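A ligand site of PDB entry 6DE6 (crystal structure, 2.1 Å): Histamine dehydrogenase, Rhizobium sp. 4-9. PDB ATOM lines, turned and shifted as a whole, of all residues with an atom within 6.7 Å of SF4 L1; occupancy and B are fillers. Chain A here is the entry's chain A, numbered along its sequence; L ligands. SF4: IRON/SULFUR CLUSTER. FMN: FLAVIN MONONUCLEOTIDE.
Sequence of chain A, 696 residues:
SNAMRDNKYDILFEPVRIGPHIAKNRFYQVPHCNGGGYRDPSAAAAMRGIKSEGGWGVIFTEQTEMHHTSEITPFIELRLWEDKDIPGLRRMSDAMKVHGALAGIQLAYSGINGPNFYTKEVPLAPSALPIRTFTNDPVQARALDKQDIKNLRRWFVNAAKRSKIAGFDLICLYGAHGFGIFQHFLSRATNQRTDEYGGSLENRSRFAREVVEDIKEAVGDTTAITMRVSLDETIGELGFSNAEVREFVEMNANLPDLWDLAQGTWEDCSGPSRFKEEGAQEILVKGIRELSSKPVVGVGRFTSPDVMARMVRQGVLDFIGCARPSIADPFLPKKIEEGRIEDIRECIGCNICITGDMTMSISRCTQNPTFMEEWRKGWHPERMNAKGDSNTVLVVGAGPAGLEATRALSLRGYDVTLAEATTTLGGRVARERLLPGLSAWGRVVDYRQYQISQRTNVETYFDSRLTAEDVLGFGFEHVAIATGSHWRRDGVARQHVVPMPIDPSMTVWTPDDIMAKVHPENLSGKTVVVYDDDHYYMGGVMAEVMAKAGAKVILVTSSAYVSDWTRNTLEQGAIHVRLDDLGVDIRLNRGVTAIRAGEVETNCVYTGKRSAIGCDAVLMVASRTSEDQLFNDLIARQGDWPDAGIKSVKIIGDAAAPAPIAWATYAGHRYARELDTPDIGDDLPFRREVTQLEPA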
ATOM      1  N   ARG A 301     -13.882   2.115  -6.395  1.00  0.00           N
ATOM      2  CA  ARG A 301     -12.943   3.232  -6.577  1.00  0.00           C
ATOM      3  C   ARG A 301     -11.515   2.800  -6.247  1.00  0.00           C
ATOM      4  O   ARG A 301     -10.793   3.414  -5.458  1.00  0.00           O
ATOM      5  CB  ARG A 301     -13.368   4.449  -5.748  1.00  0.00           C
ATOM      6  CG  ARG A 301     -12.824   5.781  -6.250  1.00  0.00           C
ATOM      7  CD  ARG A 301     -13.469   6.965  -5.541  1.00  0.00           C
ATOM      8  NE  ARG A 301     -12.983   7.069  -4.163  1.00  0.00           N
ATOM      9  CZ  ARG A 301     -13.703   6.901  -3.053  1.00  0.00           C
ATOM     10  NH1 ARG A 301     -15.025   6.638  -3.101  1.00  0.00           N
ATOM     11  NH2 ARG A 301     -13.089   7.022  -1.883  1.00  0.00           N
ATOM     12  N   ALA A 323     -13.586   2.234 -13.148  1.00  0.00           N
ATOM     13  CA  ALA A 323     -14.033   3.281 -14.045  1.00  0.00           C
ATOM     14  C   ALA A 323     -13.255   4.545 -13.718  1.00  0.00           C
ATOM     15  O   ALA A 323     -12.275   4.870 -14.391  1.00  0.00           O
ATOM     16  CB  ALA A 323     -15.539   3.474 -13.923  1.00  0.00           C
ATOM     17  N   ARG A 324     -13.629   5.236 -12.647  1.00  0.00           N
ATOM     18  CA  ARG A 324     -12.987   6.509 -12.350  1.00  0.00           C
ATOM     19  C   ARG A 324     -11.483   6.409 -12.113  1.00  0.00           C
ATOM     20  O   ARG A 324     -10.748   7.311 -12.568  1.00  0.00           O
ATOM     21  CB  ARG A 324     -13.677   7.153 -11.144  1.00  0.00           C
ATOM     22  CG  ARG A 324     -15.096   7.661 -11.482  1.00  0.00           C
ATOM     23  CD  ARG A 324     -15.879   8.015 -10.258  1.00  0.00           C
ATOM     24  NE  ARG A 324     -15.995   6.866  -9.383  1.00  0.00           N
ATOM     25  CZ  ARG A 324     -16.345   6.928  -8.098  1.00  0.00           C
ATOM     26  NH1 ARG A 324     -16.624   8.111  -7.533  1.00  0.00           N
ATOM     27  NH2 ARG A 324     -16.375   5.828  -7.388  1.00  0.00           N
ATOM     28  N   PRO A 325     -10.945   5.377 -11.452  1.00  0.00           N
ATOM     29  CA  PRO A 325      -9.473   5.282 -11.324  1.00  0.00           C
ATOM     30  C   PRO A 325      -8.750   5.196 -12.661  1.00  0.00           C
ATOM     31  O   PRO A 325      -7.590   5.631 -12.760  1.00  0.00           O
ATOM     32  CB  PRO A 325      -9.260   4.012 -10.501  1.00  0.00           C
ATOM     33  CG  PRO A 325     -10.574   3.842  -9.706  1.00  0.00           C
ATOM     34  CD  PRO A 325     -11.652   4.368 -10.634  1.00  0.00           C
ATOM     35  N   SER A 326      -9.390   4.625 -13.688  1.00  0.00           N
ATOM     36  CA  SER A 326      -8.801   4.551 -15.023  1.00  0.00           C
ATOM     37  C   SER A 326      -8.944   5.867 -15.789  1.00  0.00           C
ATOM     38  O   SER A 326      -8.166   6.104 -16.732  1.00  0.00           O
ATOM     39  CB  SER A 326      -9.462   3.421 -15.824  1.00  0.00           C
ATOM     40  OG  SER A 326     -10.739   3.796 -16.316  1.00  0.00           O
ATOM     41  N   ILE A 327      -9.916   6.700 -15.421  1.00  0.00           N
ATOM     42  CA  ILE A 327     -10.010   8.043 -15.972  1.00  0.00           C
ATOM     43  C   ILE A 327      -8.926   8.945 -15.387  1.00  0.00           C
ATOM     44  O   ILE A 327      -8.206   9.639 -16.103  1.00  0.00           O
ATOM     45  CB  ILE A 327     -11.422   8.619 -15.713  1.00  0.00           C
ATOM     46  CG1 ILE A 327     -12.456   7.817 -16.470  1.00  0.00           C
ATOM     47  CG2 ILE A 327     -11.478  10.121 -16.080  1.00  0.00           C
ATOM     48  CD1 ILE A 327     -13.889   8.084 -16.015  1.00  0.00           C
ATOM     49  N   ALA A 328      -8.786   8.929 -14.066  1.00  0.00           N
ATOM     50  CA  ALA A 328      -7.750   9.716 -13.391  1.00  0.00           C
ATOM     51  C   ALA A 328      -6.355   9.253 -13.785  1.00  0.00           C
ATOM     52  O   ALA A 328      -5.451  10.086 -13.978  1.00  0.00           O
ATOM     53  CB  ALA A 328      -7.911   9.629 -11.871  1.00  0.00           C
ATOM     54  N   ASP A 329      -6.146   7.948 -13.905  1.00  0.00           N
ATOM     55  CA  ASP A 329      -4.853   7.421 -14.322  1.00  0.00           C
ATOM     56  C   ASP A 329      -5.030   6.263 -15.284  1.00  0.00           C
ATOM     57  O   ASP A 329      -5.060   5.094 -14.861  1.00  0.00           O
ATOM     58  CB  ASP A 329      -4.021   6.971 -13.120  1.00  0.00           C
ATOM     59  CG  ASP A 329      -2.563   6.823 -13.477  1.00  0.00           C
ATOM     60  OD1 ASP A 329      -2.256   6.596 -14.671  1.00  0.00           O
ATOM     61  OD2 ASP A 329      -1.738   6.952 -12.547  1.00  0.00           O
ATOM     62  N   GLU A 346      -4.018   9.358  -8.284  1.00  0.00           N
ATOM     63  CA  GLU A 346      -5.154   8.732  -7.629  1.00  0.00           C
ATOM     64  C   GLU A 346      -6.414   9.549  -7.826  1.00  0.00           C
ATOM     65  O   GLU A 346      -6.440  10.744  -7.502  1.00  0.00           O
ATOM     66  CB  GLU A 346      -4.900   8.572  -6.131  1.00  0.00           C
ATOM     67  CG  GLU A 346      -3.750   7.670  -5.754  1.00  0.00           C
ATOM     68  CD  GLU A 346      -3.486   7.671  -4.242  1.00  0.00           C
ATOM     69  OE1 GLU A 346      -3.448   8.754  -3.660  1.00  0.00           O
ATOM     70  OE2 GLU A 346      -3.349   6.595  -3.648  1.00  0.00           O
ATOM     71  N   CYS A 347      -7.490   8.869  -8.233  1.00  0.00           N
ATOM     72  CA  CYS A 347      -8.825   9.473  -8.264  1.00  0.00           C
ATOM     73  C   CYS A 347      -9.224  10.037  -6.903  1.00  0.00           C
ATOM     74  O   CYS A 347      -9.018   9.406  -5.860  1.00  0.00           O
ATOM     75  CB  CYS A 347      -9.832   8.404  -8.711  1.00  0.00           C
ATOM     76  SG  CYS A 347     -11.553   8.924  -8.674  1.00  0.00           S
ATOM     77  N   ILE A 348      -9.811  11.229  -6.897  1.00  0.00           N
ATOM     78  CA  ILE A 348     -10.220  11.887  -5.670  1.00  0.00           C
ATOM     79  C   ILE A 348     -11.692  11.723  -5.381  1.00  0.00           C
ATOM     80  O   ILE A 348     -12.153  12.198  -4.331  1.00  0.00           O
ATOM     81  CB  ILE A 348      -9.871  13.397  -5.702  1.00  0.00           C
ATOM     82  CG1 ILE A 348     -10.742  14.139  -6.715  1.00  0.00           C
ATOM     83  CG2 ILE A 348      -8.416  13.608  -5.984  1.00  0.00           C
ATOM     84  CD1 ILE A 348     -10.457  15.647  -6.792  1.00  0.00           C
ATOM     85  N   GLY A 349     -12.455  11.070  -6.271  1.00  0.00           N
ATOM     86  CA  GLY A 349     -13.850  10.814  -5.997  1.00  0.00           C
ATOM     87  C   GLY A 349     -14.720  12.048  -5.941  1.00  0.00           C
ATOM     88  O   GLY A 349     -15.639  12.106  -5.128  1.00  0.00           O
ATOM     89  N   CYS A 350     -14.387  13.068  -6.738  1.00  0.00           N
ATOM     90  CA  CYS A 350     -15.166  14.310  -6.857  1.00  0.00           C
ATOM     91  C   CYS A 350     -16.364  14.180  -7.797  1.00  0.00           C
ATOM     92  O   CYS A 350     -17.260  15.038  -7.760  1.00  0.00           O
ATOM     93  CB  CYS A 350     -14.298  15.448  -7.382  1.00  0.00           C
ATOM     94  SG  CYS A 350     -13.603  15.114  -9.055  1.00  0.00           S
ATOM     95  N   ASN A 351     -16.352  13.169  -8.664  1.00  0.00           N
ATOM     96  CA  ASN A 351     -17.398  12.895  -9.644  1.00  0.00           C
ATOM     97  C   ASN A 351     -17.581  14.028 -10.646  1.00  0.00           C
ATOM     98  O   ASN A 351     -18.646  14.157 -11.257  1.00  0.00           O
ATOM     99  CB  ASN A 351     -18.727  12.569  -8.946  1.00  0.00           C
ATOM    100  CG  ASN A 351     -18.789  11.121  -8.461  1.00  0.00           C
ATOM    101  OD1 ASN A 351     -17.837  10.365  -8.659  1.00  0.00           O
ATOM    102  ND2 ASN A 351     -19.892  10.757  -7.806  1.00  0.00           N
ATOM    103  N   ILE A 352     -16.546  14.846 -10.881  1.00  0.00           N
ATOM    104  CA  ILE A 352     -16.640  15.867 -11.927  1.00  0.00           C
ATOM    105  C   ILE A 352     -16.837  15.215 -13.287  1.00  0.00           C
ATOM    106  O   ILE A 352     -17.539  15.756 -14.142  1.00  0.00           O
ATOM    107  CB  ILE A 352     -15.413  16.812 -11.904  1.00  0.00           C
ATOM    108  CG1 ILE A 352     -15.617  17.931 -10.863  1.00  0.00           C
ATOM    109  CG2 ILE A 352     -15.119  17.398 -13.298  1.00  0.00           C
ATOM    110  CD1 ILE A 352     -16.774  18.887 -11.190  1.00  0.00           C
ATOM    111  N   CYS A 353     -16.258  14.019 -13.488  1.00  0.00           N
ATOM    112  CA  CYS A 353     -16.412  13.260 -14.738  1.00  0.00           C
ATOM    113  C   CYS A 353     -17.869  12.971 -15.061  1.00  0.00           C
ATOM    114  O   CYS A 353     -18.278  12.996 -16.246  1.00  0.00           O
ATOM    115  CB  CYS A 353     -15.619  11.949 -14.627  1.00  0.00           C
ATOM    116  SG  CYS A 353     -15.836  11.062 -13.055  1.00  0.00           S
ATOM    117  N   ILE A 354     -18.677  12.676 -14.043  1.00  0.00           N
ATOM    118  CA  ILE A 354     -20.101  12.395 -14.236  1.00  0.00           C
ATOM    119  C   ILE A 354     -20.831  13.643 -14.681  1.00  0.00           C
ATOM    120  O   ILE A 354     -21.831  13.554 -15.414  1.00  0.00           O
ATOM    121  CB  ILE A 354     -20.673  11.802 -12.934  1.00  0.00           C
ATOM    122  CG1 ILE A 354     -20.007  10.450 -12.677  1.00  0.00           C
ATOM    123  CG2 ILE A 354     -22.211  11.628 -13.007  1.00  0.00           C
ATOM    124  CD1 ILE A 354     -20.412   9.813 -11.390  1.00  0.00           C
ATOM    125  N   ARG A 364     -14.667  15.966 -18.178  1.00  0.00           N
ATOM    126  CA  ARG A 364     -13.396  16.368 -17.619  1.00  0.00           C
ATOM    127  C   ARG A 364     -13.029  15.392 -16.513  1.00  0.00           C
ATOM    128  O   ARG A 364     -13.877  14.659 -15.990  1.00  0.00           O
ATOM    129  CB  ARG A 364     -13.481  17.762 -16.979  1.00  0.00           C
ATOM    130  CG  ARG A 364     -13.978  18.872 -17.794  1.00  0.00           C
ATOM    131  CD  ARG A 364     -14.124  20.086 -16.862  1.00  0.00           C
ATOM    132  NE  ARG A 364     -14.358  21.358 -17.546  1.00  0.00           N
ATOM    133  CZ  ARG A 364     -13.417  22.224 -17.905  1.00  0.00           C
ATOM    134  NH1 ARG A 364     -12.125  21.985 -17.674  1.00  0.00           N
ATOM    135  NH2 ARG A 364     -13.775  23.347 -18.495  1.00  0.00           N
ATOM    136  N   CYS A 365     -11.756  15.440 -16.130  1.00  0.00           N
ATOM    137  CA  CYS A 365     -11.274  14.799 -14.915  1.00  0.00           C
ATOM    138  C   CYS A 365     -10.421  15.797 -14.155  1.00  0.00           C
ATOM    139  O   CYS A 365      -9.482  16.369 -14.711  1.00  0.00           O
ATOM    140  CB  CYS A 365     -10.455  13.535 -15.228  1.00  0.00           C
ATOM    141  SG  CYS A 365      -9.669  12.804 -13.752  1.00  0.00           S
ATOM    142  N   THR A 366     -10.732  15.975 -12.870  1.00  0.00           N
ATOM    143  CA  THR A 366      -9.988  16.923 -12.032  1.00  0.00           C
ATOM    144  C   THR A 366      -8.508  16.586 -11.976  1.00  0.00           C
ATOM    145  O   THR A 366      -7.656  17.469 -12.108  1.00  0.00           O
ATOM    146  CB  THR A 366     -10.572  16.930 -10.624  1.00  0.00           C
ATOM    147  OG1 THR A 366     -11.960  17.266 -10.660  1.00  0.00           O
ATOM    148  CG2 THR A 366      -9.812  17.957  -9.782  1.00  0.00           C
ATOM    149  N   GLN A 367      -8.187  15.291 -11.795  1.00  0.00           N
ATOM    150  CA  GLN A 367      -6.807  14.829 -11.732  1.00  0.00           C
ATOM    151  C   GLN A 367      -6.141  14.776 -13.101  1.00  0.00           C
ATOM    152  O   GLN A 367      -4.955  15.113 -13.226  1.00  0.00           O
ATOM    153  CB  GLN A 367      -6.755  13.425 -11.099  1.00  0.00           C
ATOM    154  CG  GLN A 367      -6.744  13.433  -9.571  1.00  0.00           C
ATOM    155  CD  GLN A 367      -5.418  13.907  -8.978  1.00  0.00           C
ATOM    156  OE1 GLN A 367      -4.921  14.972  -9.319  1.00  0.00           O
ATOM    157  NE2 GLN A 367      -4.887  13.139  -8.039  1.00  0.00           N
ATOM    158  N   ASN A 368      -6.862  14.358 -14.134  1.00  0.00           N
ATOM    159  CA  ASN A 368      -6.276  14.075 -15.441  1.00  0.00           C
ATOM    160  C   ASN A 368      -6.889  15.000 -16.478  1.00  0.00           C
ATOM    161  O   ASN A 368      -7.839  14.635 -17.182  1.00  0.00           O
ATOM    162  CB  ASN A 368      -6.494  12.622 -15.841  1.00  0.00           C
ATOM    163  CG  ASN A 368      -5.944  12.334 -17.218  1.00  0.00           C
ATOM    164  OD1 ASN A 368      -5.115  13.093 -17.745  1.00  0.00           O
ATOM    165  ND2 ASN A 368      -6.434  11.278 -17.837  1.00  0.00           N
ATOM    166  N   VAL A 444      -4.836  15.997  -5.298  1.00  0.00           N
ATOM    167  CA  VAL A 444      -4.509  16.892  -6.415  1.00  0.00           C
ATOM    168  C   VAL A 444      -3.181  17.598  -6.168  1.00  0.00           C
ATOM    169  O   VAL A 444      -2.362  17.755  -7.082  1.00  0.00           O
ATOM    170  CB  VAL A 444      -5.655  17.912  -6.596  1.00  0.00           C
ATOM    171  CG1 VAL A 444      -5.241  19.056  -7.497  1.00  0.00           C
ATOM    172  CG2 VAL A 444      -6.875  17.211  -7.147  1.00  0.00           C
ATOM    173  N   ALA A 662     -11.097  21.440 -11.197  1.00  0.00           N
ATOM    174  CA  ALA A 662     -10.739  20.797 -12.456  1.00  0.00           C
ATOM    175  C   ALA A 662     -10.476  21.831 -13.535  1.00  0.00           C
ATOM    176  O   ALA A 662      -9.645  21.596 -14.420  1.00  0.00           O
ATOM    177  CB  ALA A 662     -11.834  19.836 -12.901  1.00  0.00           C
HETATM  178 FE1  SF4 L   1     -11.327  12.342 -12.196  1.00  0.00          FE
HETATM  179 FE2  SF4 L   1     -13.900  11.464 -11.868  1.00  0.00          FE
HETATM  180 FE3  SF4 L   1     -12.798  13.181  -9.982  1.00  0.00          FE
HETATM  181 FE4  SF4 L   1     -11.873  10.647 -10.151  1.00  0.00          FE
HETATM  182  S1  SF4 L   1     -13.981  11.290  -9.564  1.00  0.00           S
HETATM  183  S2  SF4 L   1     -10.564  12.554 -10.050  1.00  0.00           S
HETATM  184  S3  SF4 L   1     -12.077  10.215 -12.371  1.00  0.00           S
HETATM  185  S4  SF4 L   1     -13.232  13.653 -12.182  1.00  0.00           S
HETATM  186  N1  FMN L   2     -21.706   1.959 -15.815  1.00  0.00           N
HETATM  187  C2  FMN L   2     -22.287   1.163 -16.882  1.00  0.00           C
HETATM  188  O2  FMN L   2     -22.519   0.013 -16.688  1.00  0.00           O
HETATM  189  N3  FMN L   2     -22.606   1.818 -18.175  1.00  0.00           N
HETATM  190  C4  FMN L   2     -22.306   3.217 -18.402  1.00  0.00           C
HETATM  191  O4  FMN L   2     -22.555   3.741 -19.435  1.00  0.00           O
HETATM  192  C4A FMN L   2     -21.691   4.006 -17.287  1.00  0.00           C
HETATM  193  N5  FMN L   2     -21.385   5.398 -17.483  1.00  0.00           N
HETATM  194  C5A FMN L   2     -20.732   6.177 -16.380  1.00  0.00           C
HETATM  195  C6  FMN L   2     -20.135   7.421 -16.707  1.00  0.00           C
HETATM  196  C7  FMN L   2     -19.097   7.903 -15.891  1.00  0.00           C
HETATM  197  C7M FMN L   2     -18.659   9.315 -16.273  1.00  0.00           C
HETATM  198  C8  FMN L   2     -18.759   7.205 -14.718  1.00  0.00           C
HETATM  199  C8M FMN L   2     -17.693   7.777 -13.772  1.00  0.00           C
HETATM  200  C9  FMN L   2     -19.403   6.031 -14.379  1.00  0.00           C
HETATM  201  C9A FMN L   2     -20.436   5.520 -15.174  1.00  0.00           C
HETATM  202  N10 FMN L   2     -20.772   4.087 -14.975  1.00  0.00           N
HETATM  203  C10 FMN L   2     -21.394   3.352 -16.040  1.00  0.00           C
HETATM  204  C1' FMN L   2     -20.517   3.390 -13.718  1.00  0.00           C
HETATM  205  C2' FMN L   2     -19.112   2.797 -13.681  1.00  0.00           C
HETATM  206  O2' FMN L   2     -19.044   1.758 -14.608  1.00  0.00           O
HETATM  207  C3' FMN L   2     -18.751   2.223 -12.307  1.00  0.00           C
HETATM  208  O3' FMN L   2     -19.663   1.196 -11.985  1.00  0.00           O
HETATM  209  C4' FMN L   2     -18.786   3.304 -11.198  1.00  0.00           C
HETATM  210  O4' FMN L   2     -18.177   4.539 -11.564  1.00  0.00           O
HETATM  211  C5' FMN L   2     -18.064   2.728  -9.949  1.00  0.00           C
HETATM  212  O5' FMN L   2     -16.799   2.187 -10.271  1.00  0.00           O
HETATM  213  P   FMN L   2     -15.443   3.063  -9.954  1.00  0.00           P
HETATM  214  O1P FMN L   2     -15.575   4.372 -10.718  1.00  0.00           O
HETATM  215  O2P FMN L   2     -15.416   3.274  -8.451  1.00  0.00           O
HETATM  216  O3P FMN L   2     -14.243   2.268 -10.343  1.00  0.00           O
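O of Arg 324 sits close to S3 of SF4 L1, 3.2 Å away. CG2 of Ile 327 touches S3 of SF4 L1, at 3.8 Å. N of Ala 328 touches S3 of SF4 L1, at 3.9 Å. O of Arg 364 touches S4 of SF4 L1, at 3.99 Å. Gln 367 touches SF4 L1. Hydrophobic or aromatic side chains within 4 Å of SF4 L1: Ile 327, Ile 348 and Ile 352. The nearest printed residue that does not touch SF4 L1 is Pro 325 (5.1 Å).
The backbone NH (N) of Cys 350 lies close to a sulfur (S1) of SF4 L1. The backbone NH of Ala 323 is in hydrogen-bond range of an oxygen (O3P) of FMN L2, 2.9 Å away. The side-chain sulfur of Cys 365 binds an iron atom (FE1) of SF4 L1 (2.3 Å). SG of Cys 347 is bound to FE4 of SF4 L1. The backbone NH (N) of Thr 366 lies close to a sulfur (S4) of SF4 L1, 3.5 Å away. An iron atom (FE2) of SF4 L1 is bound by the side-chain sulfur of Cys 353 (2.3 Å). The backbone NH (N) of Asn 351 sits close to a sulfur (S1) of SF4 L1, 3.2 Å away. A sulfur (S4) of SF4 L1 sits close to the backbone NH (N) of Cys 353. The backbone NH (N) of Ile 348 lies close to a sulfur (S2) of SF4 L1 (3.5 Å). O2P of FMN L2 is in hydrogen-bond range of N of Arg 301 (2.8 Å). SG of Cys 350 is bound to FE3 of SF4 L1 (2.3 Å). The backbone NH of Ile 352 sits close to a sulfur (S4) of SF4 L1. An oxygen (O1P) of FMN L2 is in salt-bridge range of the guanidinium group (NE) of Arg 324 (2.9 Å). The backbone NH (N) of Arg 324 is in hydrogen-bond range of an oxygen (O1P) of FMN L2, at 2.9 Å. A sulfur (S1) of SF4 L1 sits close to the backbone NH (N) of Gly 349 (3.6 Å).
The side-chain sulfur (SG) of Cys 350 lies close to the backbone NH (N) of Ile 352, 3.5 Å away. The backbone NH (N) of Gln 367 sits close to the side-chain sulfur (SG) of Cys 365. O of Ile 327 lies within hydrogen-bond range of ND2 of Asn 368, at 3.0 Å. SG of Cys 347 sits close to N of Gly 349 (3.3 Å). NE2 of Gln 367 is in hydrogen-bond range of O of Glu 346, 2.9 Å away. The side-chain amide oxygen (OD1) of Asn 351 lies within hydrogen-bond range of the guanidinium group (NH1) of Arg 324 (2.8 Å). The side-chain hydroxyl of Thr 366 sits close to the side-chain sulfur of Cys 350 (3.1 Å). The backbone NH (N) of Asn 368 lies close to the side-chain sulfur (SG) of Cys 365, 3.2 Å away.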
